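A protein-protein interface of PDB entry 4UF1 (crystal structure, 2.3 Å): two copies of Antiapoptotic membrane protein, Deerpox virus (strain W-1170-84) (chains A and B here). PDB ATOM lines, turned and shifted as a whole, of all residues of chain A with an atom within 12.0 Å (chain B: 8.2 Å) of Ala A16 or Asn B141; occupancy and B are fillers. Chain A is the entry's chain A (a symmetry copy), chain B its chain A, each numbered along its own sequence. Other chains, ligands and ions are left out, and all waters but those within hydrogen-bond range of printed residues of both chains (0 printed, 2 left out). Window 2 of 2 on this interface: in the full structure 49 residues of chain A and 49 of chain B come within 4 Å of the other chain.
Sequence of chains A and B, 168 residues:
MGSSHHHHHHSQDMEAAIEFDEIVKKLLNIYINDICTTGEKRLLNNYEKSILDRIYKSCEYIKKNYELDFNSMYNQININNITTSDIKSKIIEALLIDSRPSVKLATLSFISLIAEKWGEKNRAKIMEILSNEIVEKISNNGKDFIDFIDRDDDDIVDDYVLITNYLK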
ATOM      1  N   ALA A  16     -11.138 -17.617 -12.742  1.00  0.00           N
ATOM      2  CA  ALA A  16     -10.627 -16.358 -12.213  1.00  0.00           C
ATOM      3  C   ALA A  16     -11.195 -16.099 -10.817  1.00  0.00           C
ATOM      4  O   ALA A  16     -10.738 -16.696  -9.841  1.00  0.00           O
ATOM      5  CB  ALA A  16     -10.961 -15.213 -13.161  1.00  0.00           C
ATOM      6  N   ALA A  17     -12.184 -15.213 -10.723  1.00  0.00           N
ATOM      7  CA  ALA A  17     -12.866 -14.945  -9.461  1.00  0.00           C
ATOM      8  C   ALA A  17     -14.169 -15.728  -9.411  1.00  0.00           C
ATOM      9  O   ALA A  17     -15.126 -15.402 -10.110  1.00  0.00           O
ATOM     10  CB  ALA A  17     -13.129 -13.462  -9.297  1.00  0.00           C
ATOM     11  N   ILE A  18     -14.196 -16.757  -8.574  1.00  0.00           N
ATOM     12  CA  ILE A  18     -15.311 -17.693  -8.530  1.00  0.00           C
ATOM     13  C   ILE A  18     -16.191 -17.488  -7.299  1.00  0.00           C
ATOM     14  O   ILE A  18     -17.212 -18.161  -7.144  1.00  0.00           O
ATOM     15  CB  ILE A  18     -14.799 -19.150  -8.533  1.00  0.00           C
ATOM     16  CG1 ILE A  18     -14.026 -19.453  -7.243  1.00  0.00           C
ATOM     17  CG2 ILE A  18     -13.909 -19.391  -9.747  1.00  0.00           C
ATOM     18  CD1 ILE A  18     -13.713 -20.920  -7.040  1.00  0.00           C
ATOM     19  N   GLU A  19     -15.802 -16.555  -6.432  1.00  0.00           N
ATOM     20  CA  GLU A  19     -16.365 -16.497  -5.083  1.00  0.00           C
ATOM     21  C   GLU A  19     -17.825 -16.015  -5.041  1.00  0.00           C
ATOM     22  O   GLU A  19     -18.458 -16.061  -3.981  1.00  0.00           O
ATOM     23  CB  GLU A  19     -15.488 -15.610  -4.181  1.00  0.00           C
ATOM     24  CG  GLU A  19     -15.543 -14.116  -4.472  1.00  0.00           C
ATOM     25  CD  GLU A  19     -14.348 -13.609  -5.266  1.00  0.00           C
ATOM     26  OE1 GLU A  19     -13.759 -14.392  -6.040  1.00  0.00           O
ATOM     27  OE2 GLU A  19     -13.996 -12.417  -5.112  1.00  0.00           O
ATOM     28  N   PHE A  20     -18.358 -15.564  -6.177  1.00  0.00           N
ATOM     29  CA  PHE A  20     -19.767 -15.163  -6.263  1.00  0.00           C
ATOM     30  C   PHE A  20     -20.587 -16.086  -7.167  1.00  0.00           C
ATOM     31  O   PHE A  20     -21.757 -15.816  -7.430  1.00  0.00           O
ATOM     32  CB  PHE A  20     -19.891 -13.722  -6.775  1.00  0.00           C
ATOM     33  CG  PHE A  20     -19.443 -12.685  -5.789  1.00  0.00           C
ATOM     34  CD1 PHE A  20     -20.338 -12.136  -4.888  1.00  0.00           C
ATOM     35  CD2 PHE A  20     -18.129 -12.253  -5.769  1.00  0.00           C
ATOM     36  CE1 PHE A  20     -19.927 -11.181  -3.980  1.00  0.00           C
ATOM     37  CE2 PHE A  20     -17.709 -11.300  -4.863  1.00  0.00           C
ATOM     38  CZ  PHE A  20     -18.606 -10.762  -3.969  1.00  0.00           C
ATOM     39  N   ASP A  21     -19.980 -17.169  -7.640  1.00  0.00           N
ATOM     40  CA  ASP A  21     -20.655 -18.071  -8.567  1.00  0.00           C
ATOM     41  C   ASP A  21     -21.919 -18.689  -7.966  1.00  0.00           C
ATOM     42  O   ASP A  21     -22.964 -18.723  -8.610  1.00  0.00           O
ATOM     43  CB  ASP A  21     -19.705 -19.180  -9.014  1.00  0.00           C
ATOM     44  CG  ASP A  21     -18.639 -18.683  -9.973  1.00  0.00           C
ATOM     45  OD1 ASP A  21     -18.401 -17.457 -10.016  1.00  0.00           O
ATOM     46  OD2 ASP A  21     -18.035 -19.518 -10.680  1.00  0.00           O
ATOM     47  N   GLU A  22     -21.820 -19.176  -6.734  1.00  0.00           N
ATOM     48  CA  GLU A  22     -22.944 -19.843  -6.086  1.00  0.00           C
ATOM     49  C   GLU A  22     -24.070 -18.867  -5.745  1.00  0.00           C
ATOM     50  O   GLU A  22     -25.244 -19.233  -5.772  1.00  0.00           O
ATOM     51  CB  GLU A  22     -22.474 -20.563  -4.821  1.00  0.00           C
ATOM     52  CG  GLU A  22     -21.580 -21.759  -5.094  1.00  0.00           C
ATOM     53  CD  GLU A  22     -22.268 -22.823  -5.929  1.00  0.00           C
ATOM     54  OE1 GLU A  22     -23.466 -23.085  -5.684  1.00  0.00           O
ATOM     55  OE2 GLU A  22     -21.616 -23.388  -6.834  1.00  0.00           O
ATOM     56  N   ILE A  23     -23.714 -17.628  -5.424  1.00  0.00           N
ATOM     57  CA  ILE A  23     -24.712 -16.600  -5.138  1.00  0.00           C
ATOM     58  C   ILE A  23     -25.542 -16.316  -6.382  1.00  0.00           C
ATOM     59  O   ILE A  23     -26.767 -16.238  -6.311  1.00  0.00           O
ATOM     60  CB  ILE A  23     -24.055 -15.294  -4.635  1.00  0.00           C
ATOM     61  CG1 ILE A  23     -23.559 -15.487  -3.199  1.00  0.00           C
ATOM     62  CG2 ILE A  23     -25.045 -14.124  -4.691  1.00  0.00           C
ATOM     63  CD1 ILE A  23     -22.743 -14.333  -2.647  1.00  0.00           C
ATOM     64  N   VAL A  24     -24.875 -16.171  -7.522  1.00  0.00           N
ATOM     65  CA  VAL A  24     -25.572 -15.894  -8.771  1.00  0.00           C
ATOM     66  C   VAL A  24     -26.525 -17.044  -9.093  1.00  0.00           C
ATOM     67  O   VAL A  24     -27.697 -16.816  -9.373  1.00  0.00           O
ATOM     68  CB  VAL A  24     -24.582 -15.670  -9.937  1.00  0.00           C
ATOM     69  CG1 VAL A  24     -25.302 -15.683 -11.284  1.00  0.00           C
ATOM     70  CG2 VAL A  24     -23.844 -14.356  -9.750  1.00  0.00           C
ATOM     71  N   LYS A  25     -26.024 -18.273  -9.030  1.00  0.00           N
ATOM     72  CA  LYS A  25     -26.846 -19.448  -9.306  1.00  0.00           C
ATOM     73  C   LYS A  25     -28.077 -19.500  -8.401  1.00  0.00           C
ATOM     74  O   LYS A  25     -29.182 -19.804  -8.855  1.00  0.00           O
ATOM     75  CB  LYS A  25     -26.021 -20.729  -9.145  1.00  0.00           C
ATOM     76  CG  LYS A  25     -26.861 -21.988  -8.942  1.00  0.00           C
ATOM     77  CD  LYS A  25     -26.123 -23.254  -9.356  1.00  0.00           C
ATOM     78  CE  LYS A  25     -24.670 -23.246  -8.909  1.00  0.00           C
ATOM     79  NZ  LYS A  25     -24.066 -24.606  -8.958  1.00  0.00           N
ATOM     80  N   LYS A  26     -27.885 -19.195  -7.123  1.00  0.00           N
ATOM     81  CA  LYS A  26     -28.984 -19.231  -6.162  1.00  0.00           C
ATOM     82  C   LYS A  26     -30.032 -18.162  -6.460  1.00  0.00           C
ATOM     83  O   LYS A  26     -31.228 -18.435  -6.433  1.00  0.00           O
ATOM     84  CB  LYS A  26     -28.453 -19.055  -4.738  1.00  0.00           C
ATOM     85  CG  LYS A  26     -29.542 -18.974  -3.674  1.00  0.00           C
ATOM     86  CD  LYS A  26     -28.947 -18.883  -2.282  1.00  0.00           C
ATOM     87  CE  LYS A  26     -29.955 -19.260  -1.209  1.00  0.00           C
ATOM     88  NZ  LYS A  26     -29.404 -20.298  -0.294  1.00  0.00           N
ATOM     89  N   LEU A  28     -30.594 -16.638  -9.279  1.00  0.00           N
ATOM     90  CA  LEU A  28     -31.227 -16.845 -10.579  1.00  0.00           C
ATOM     91  C   LEU A  28     -32.371 -17.852 -10.480  1.00  0.00           C
ATOM     92  O   LEU A  28     -33.386 -17.701 -11.153  1.00  0.00           O
ATOM     93  CB  LEU A  28     -30.205 -17.312 -11.621  1.00  0.00           C
ATOM     94  CG  LEU A  28     -29.199 -16.279 -12.150  1.00  0.00           C
ATOM     95  CD1 LEU A  28     -28.456 -16.852 -13.343  1.00  0.00           C
ATOM     96  CD2 LEU A  28     -29.850 -14.952 -12.512  1.00  0.00           C
ATOM     97  N   SER B  99     -19.457 -15.109 -23.812  1.00  0.00           N
ATOM     98  CA  SER B  99     -19.946 -15.122 -22.433  1.00  0.00           C
ATOM     99  C   SER B  99     -19.731 -13.793 -21.702  1.00  0.00           C
ATOM    100  O   SER B  99     -19.555 -13.773 -20.485  1.00  0.00           O
ATOM    101  CB  SER B  99     -19.268 -16.251 -21.653  1.00  0.00           C
ATOM    102  OG  SER B  99     -17.881 -16.008 -21.496  1.00  0.00           O
ATOM    103  N   PRO B 101     -20.948 -10.407 -19.897  1.00  0.00           N
ATOM    104  CA  PRO B 101     -22.139 -10.234 -19.056  1.00  0.00           C
ATOM    105  C   PRO B 101     -23.346  -9.649 -19.795  1.00  0.00           C
ATOM    106  O   PRO B 101     -24.480  -9.916 -19.398  1.00  0.00           O
ATOM    107  CB  PRO B 101     -21.657  -9.269 -17.967  1.00  0.00           C
ATOM    108  CG  PRO B 101     -20.197  -9.500 -17.880  1.00  0.00           C
ATOM    109  CD  PRO B 101     -19.759  -9.775 -19.294  1.00  0.00           C
ATOM    110  N   LYS B 104     -25.147 -12.514 -21.158  1.00  0.00           N
ATOM    111  CA  LYS B 104     -25.757 -13.230 -20.039  1.00  0.00           C
ATOM    112  C   LYS B 104     -27.059 -12.555 -19.644  1.00  0.00           C
ATOM    113  O   LYS B 104     -28.068 -13.220 -19.407  1.00  0.00           O
ATOM    114  CB  LYS B 104     -24.811 -13.285 -18.838  1.00  0.00           C
ATOM    115  CG  LYS B 104     -23.610 -14.196 -19.035  1.00  0.00           C
ATOM    116  CD  LYS B 104     -22.696 -14.189 -17.821  1.00  0.00           C
ATOM    117  CE  LYS B 104     -21.651 -15.287 -17.921  1.00  0.00           C
ATOM    118  NZ  LYS B 104     -20.687 -15.263 -16.793  1.00  0.00           N
ATOM    119  N   GLU B 136     -25.408 -22.586 -14.938  1.00  0.00           N
ATOM    120  CA  GLU B 136     -23.973 -22.732 -14.696  1.00  0.00           C
ATOM    121  C   GLU B 136     -23.176 -21.780 -15.578  1.00  0.00           C
ATOM    122  O   GLU B 136     -22.204 -21.176 -15.134  1.00  0.00           O
ATOM    123  CB  GLU B 136     -23.510 -24.167 -14.958  1.00  0.00           C
ATOM    124  CG  GLU B 136     -22.954 -24.879 -13.739  1.00  0.00           C
ATOM    125  CD  GLU B 136     -23.998 -25.105 -12.664  1.00  0.00           C
ATOM    126  OE1 GLU B 136     -25.054 -25.698 -12.970  1.00  0.00           O
ATOM    127  OE2 GLU B 136     -23.762 -24.687 -11.511  1.00  0.00           O
ATOM    128  N   LYS B 137     -23.593 -21.657 -16.834  1.00  0.00           N
ATOM    129  CA  LYS B 137     -22.882 -20.835 -17.805  1.00  0.00           C
ATOM    130  C   LYS B 137     -22.967 -19.360 -17.418  1.00  0.00           C
ATOM    131  O   LYS B 137     -21.996 -18.618 -17.553  1.00  0.00           O
ATOM    132  CB  LYS B 137     -23.453 -21.058 -19.211  1.00  0.00           C
ATOM    133  CG  LYS B 137     -22.555 -20.602 -20.357  1.00  0.00           C
ATOM    134  CD  LYS B 137     -21.345 -21.514 -20.555  1.00  0.00           C
ATOM    135  CE  LYS B 137     -20.793 -21.399 -21.974  1.00  0.00           C
ATOM    136  NZ  LYS B 137     -19.304 -21.384 -22.027  1.00  0.00           N
ATOM    137  N   ILE B 138     -24.131 -18.940 -16.928  1.00  0.00           N
ATOM    138  CA  ILE B 138     -24.320 -17.565 -16.466  1.00  0.00           C
ATOM    139  C   ILE B 138     -23.600 -17.330 -15.140  1.00  0.00           C
ATOM    140  O   ILE B 138     -23.014 -16.268 -14.928  1.00  0.00           O
ATOM    141  CB  ILE B 138     -25.827 -17.214 -16.298  1.00  0.00           C
ATOM    142  CG1 ILE B 138     -26.549 -17.353 -17.645  1.00  0.00           C
ATOM    143  CG2 ILE B 138     -25.996 -15.803 -15.716  1.00  0.00           C
ATOM    144  CD1 ILE B 138     -27.929 -16.699 -17.718  1.00  0.00           C
ATOM    145  N   SER B 139     -23.635 -18.325 -14.258  1.00  0.00           N
ATOM    146  CA  SER B 139     -23.070 -18.180 -12.917  1.00  0.00           C
ATOM    147  C   SER B 139     -21.543 -18.127 -12.952  1.00  0.00           C
ATOM    148  O   SER B 139     -20.918 -17.520 -12.079  1.00  0.00           O
ATOM    149  CB  SER B 139     -23.538 -19.324 -12.013  1.00  0.00           C
ATOM    150  OG  SER B 139     -24.936 -19.258 -11.811  1.00  0.00           O
ATOM    151  N   ASN B 140     -20.956 -18.781 -13.953  1.00  0.00           N
ATOM    152  CA  ASN B 140     -19.523 -18.681 -14.224  1.00  0.00           C
ATOM    153  C   ASN B 140     -19.067 -17.229 -14.189  1.00  0.00           C
ATOM    154  O   ASN B 140     -19.658 -16.378 -14.850  1.00  0.00           O
ATOM    155  CB  ASN B 140     -19.193 -19.295 -15.588  1.00  0.00           C
ATOM    156  CG  ASN B 140     -18.171 -20.403 -15.498  1.00  0.00           C
ATOM    157  OD1 ASN B 140     -18.517 -21.562 -15.267  1.00  0.00           O
ATOM    158  ND2 ASN B 140     -16.904 -20.059 -15.695  1.00  0.00           N
ATOM    159  N   ASN B 141     -18.021 -16.951 -13.415  1.00  0.00           N
ATOM    160  CA  ASN B 141     -17.539 -15.585 -13.225  1.00  0.00           C
ATOM    161  C   ASN B 141     -18.670 -14.671 -12.774  1.00  0.00           C
ATOM    162  O   ASN B 141     -18.804 -13.547 -13.254  1.00  0.00           O
ATOM    163  CB  ASN B 141     -16.904 -15.046 -14.512  1.00  0.00           C
ATOM    164  CG  ASN B 141     -15.638 -15.791 -14.892  1.00  0.00           C
ATOM    165  OD1 ASN B 141     -14.568 -15.547 -14.332  1.00  0.00           O
ATOM    166  ND2 ASN B 141     -15.753 -16.700 -15.852  1.00  0.00           N
ATOM    167  N   GLY B 142     -19.486 -15.174 -11.852  1.00  0.00           N
ATOM    168  CA  GLY B 142     -20.640 -14.448 -11.357  1.00  0.00           C
ATOM    169  C   GLY B 142     -20.308 -13.049 -10.878  1.00  0.00           C
ATOM    170  O   GLY B 142     -21.126 -12.138 -10.996  1.00  0.00           O
ATOM    171  N   LYS B 143     -19.108 -12.881 -10.338  1.00  0.00           N
ATOM    172  CA  LYS B 143     -18.669 -11.582  -9.842  1.00  0.00           C
ATOM    173  C   LYS B 143     -18.728 -10.526 -10.937  1.00  0.00           C
ATOM    174  O   LYS B 143     -19.238  -9.427 -10.722  1.00  0.00           O
ATOM    175  CB  LYS B 143     -17.250 -11.670  -9.287  1.00  0.00           C
ATOM    176  CG  LYS B 143     -16.794 -10.390  -8.603  1.00  0.00           C
ATOM    177  CD  LYS B 143     -15.381 -10.508  -8.072  1.00  0.00           C
ATOM    178  CE  LYS B 143     -14.987  -9.266  -7.301  1.00  0.00           C
ATOM    179  NZ  LYS B 143     -13.772  -9.495  -6.476  1.00  0.00           N
ATOM    180  N   ASP B 144     -18.201 -10.864 -12.110  1.00  0.00           N
ATOM    181  CA  ASP B 144     -18.229  -9.954 -13.248  1.00  0.00           C
ATOM    182  C   ASP B 144     -19.667  -9.651 -13.659  1.00  0.00           C
ATOM    183  O   ASP B 144     -19.975  -8.536 -14.076  1.00  0.00           O
ATOM    184  CB  ASP B 144     -17.455 -10.537 -14.433  1.00  0.00           C
ATOM    185  CG  ASP B 144     -15.969 -10.661 -14.156  1.00  0.00           C
ATOM    186  OD1 ASP B 144     -15.456  -9.911 -13.297  1.00  0.00           O
ATOM    187  OD2 ASP B 144     -15.316 -11.509 -14.801  1.00  0.00           O
ATOM    188  N   PHE B 145     -20.544 -10.642 -13.532  1.00  0.00           N
ATOM    189  CA  PHE B 145     -21.950 -10.444 -13.860  1.00  0.00           C
ATOM    190  C   PHE B 145     -22.597  -9.486 -12.868  1.00  0.00           C
ATOM    191  O   PHE B 145     -23.306  -8.560 -13.266  1.00  0.00           O
ATOM    192  CB  PHE B 145     -22.709 -11.773 -13.878  1.00  0.00           C
ATOM    193  CG  PHE B 145     -24.166 -11.625 -14.221  1.00  0.00           C
ATOM    194  CD1 PHE B 145     -24.552 -11.229 -15.490  1.00  0.00           C
ATOM    195  CD2 PHE B 145     -25.147 -11.877 -13.278  1.00  0.00           C
ATOM    196  CE1 PHE B 145     -25.888 -11.087 -15.811  1.00  0.00           C
ATOM    197  CE2 PHE B 145     -26.485 -11.736 -13.597  1.00  0.00           C
ATOM    198  CZ  PHE B 145     -26.852 -11.341 -14.865  1.00  0.00           C
ATOM    199  N   ILE B 146     -22.351  -9.704 -11.579  1.00  0.00           N
ATOM    200  CA  ILE B 146     -22.893  -8.826 -10.546  1.00  0.00           C
ATOM    201  C   ILE B 146     -22.377  -7.405 -10.748  1.00  0.00           C
ATOM    202  O   ILE B 146     -23.147  -6.446 -10.700  1.00  0.00           O
ATOM    203  CB  ILE B 146     -22.536  -9.319  -9.124  1.00  0.00           C
ATOM    204  CG1 ILE B 146     -23.264 -10.637  -8.830  1.00  0.00           C
ATOM    205  CG2 ILE B 146     -22.906  -8.265  -8.076  1.00  0.00           C
ATOM    206  CD1 ILE B 146     -22.991 -11.231  -7.450  1.00  0.00           C
ATOM    207  N   ASP B 147     -21.073  -7.275 -10.979  1.00  0.00           N
ATOM    208  CA  ASP B 147     -20.454  -5.973 -11.203  1.00  0.00           C
ATOM    209  C   ASP B 147     -21.089  -5.247 -12.391  1.00  0.00           C
ATOM    210  O   ASP B 147     -21.174  -4.019 -12.404  1.00  0.00           O
ATOM    211  CB  ASP B 147     -18.951  -6.132 -11.431  1.00  0.00           C
ATOM    212  CG  ASP B 147     -18.232  -4.802 -11.542  1.00  0.00           C
ATOM    213  OD1 ASP B 147     -18.007  -4.156 -10.496  1.00  0.00           O
ATOM    214  OD2 ASP B 147     -17.883  -4.405 -12.674  1.00  0.00           O
ATOM    215  N   PHE B 148     -21.540  -6.011 -13.380  1.00  0.00           N
ATOM    216  CA  PHE B 148     -22.132  -5.435 -14.582  1.00  0.00           C
ATOM    217  C   PHE B 148     -23.491  -4.792 -14.299  1.00  0.00           C
ATOM    218  O   PHE B 148     -23.798  -3.731 -14.840  1.00  0.00           O
ATOM    219  CB  PHE B 148     -22.278  -6.504 -15.668  1.00  0.00           C
ATOM    220  CG  PHE B 148     -22.767  -5.970 -16.987  1.00  0.00           C
ATOM    221  CD1 PHE B 148     -21.893  -5.358 -17.870  1.00  0.00           C
ATOM    222  CD2 PHE B 148     -24.101  -6.087 -17.345  1.00  0.00           C
ATOM    223  CE1 PHE B 148     -22.340  -4.867 -19.085  1.00  0.00           C
ATOM    224  CE2 PHE B 148     -24.556  -5.598 -18.558  1.00  0.00           C
ATOM    225  CZ  PHE B 148     -23.675  -4.988 -19.429  1.00  0.00           C
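Printed residues of chain B within 4 Å of Ala A16: Asn B141 (3.8 Å).
Of the printed residues of chain B, Asp A21 touches Ser B139 (3.3 Å), Asn B140 (3.9 Å), Asn B141 (3.5 Å) and Gly B142 (3.1 Å).
Ile A23 touches none of the printed residues of chain B.
Lys B104 touches none of the printed residues of chain A.
Of chain A, only Asp A21, Val A24 and Lys A25 come within 4 Å of Ser B139.
Asn B140 touches one residue of chain A.
Asn B141 touches just these residues of chain A: Ala A16 (3.8 Å), Ala A17 (3.9 Å) and Asp A21 (3.5 Å).
Of chain A, only Asp A21 (3.1 Å) and Val A24 (3.6 Å) come within 4 Å of Gly B142.
Of the printed residues of chain A, Lys B143 touches Ala A17, Glu A19 and Phe A20.
No residue of chain A comes within 4 Å of Asp B144.
Of the printed residues of chain A, Ile B146 touches Phe A20 (3.8 Å) and Val A24 (3.9 Å).
The nearest residue of chain A that does not touch Asn B141 is Ile A18 (5.6 Å).
The nearest printed residue of chain B that does not touch Val A24 is Phe B145 (4.3 Å).
The side-chain carboxylate (OE2) of Glu B136 is in salt-bridge range of the side-chain amino group (NZ) of Lys A25.
The backbone NH (N) of Lys A25 lies within hydrogen-bond range of the side-chain hydroxyl (OG) of Ser B139.
N of Asn B141 sits at hydrogen-bond distance from OD1 of Asp A21, at 3.5 Å.
The side-chain carboxylate (OD1) of Asp A21 sits at hydrogen-bond distance from the backbone NH (N) of Gly B142, 3.1 Å away.
The side-chain amino group (NZ) of Lys B143 lies within salt-bridge range of the side-chain carboxylate (OE2) of Glu A19 (3.2 Å).
OD1 of Asp A21 lies close to O of Ser B139 (3.3 Å).
No position is printed for both chains.
Of the 16 pairs that touch across the chains among the printed residues, none has its exchanged pair printed and touching as well.
Of the 16 printed residues of chain B, 8 touch a printed residue of chain A.
Printed residues of chain A that touch a printed residue of chain B: Ala A16, Ala A17, Glu A19, Phe A20, Asp A21, Val A24, Lys A25 and Leu A28.
Hydrophobic or aromatic side chains of chain A that line the printed part of chain B: Ala A16, Ala A17, Phe A20, Val A24 and Leu A28.
Among the printed residues, 16 pairs touch across the chains.
Among the printed residues, Asp or Glu carboxylates within 4 Å of a Lys or Arg side-chain nitrogen of the other chain: Glu A19 with Lys B143 (3.2 Å) and Lys A25 with Glu B136 (2.6 Å).
Among the printed residues, pairs that only touch across the chains: Leu A28 with Ile B138, Val A24 with Gly B142, Val A24 with Ser B139, Phe A20 with Lys B143, Phe A20 with Ile B146, Ala A16 with Asn B141, Val A24 with Ile B146, Ala A17 with Lys B143, Asp A21 with Asn B140 and Ala A17 with Asn B141.
NZ of Lys B104 lies within hydrogen-bond range of O of Ile B138 (3.1 Å).
The side-chain amino group (NZ) of Lys B104 sits at hydrogen-bond distance from the backbone carbonyl oxygen (O) of Asn B140 (2.5 Å).
The side-chain carboxylate (OE2) of Glu A22 is in salt-bridge range of the side-chain amino group (NZ) of Lys A25.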
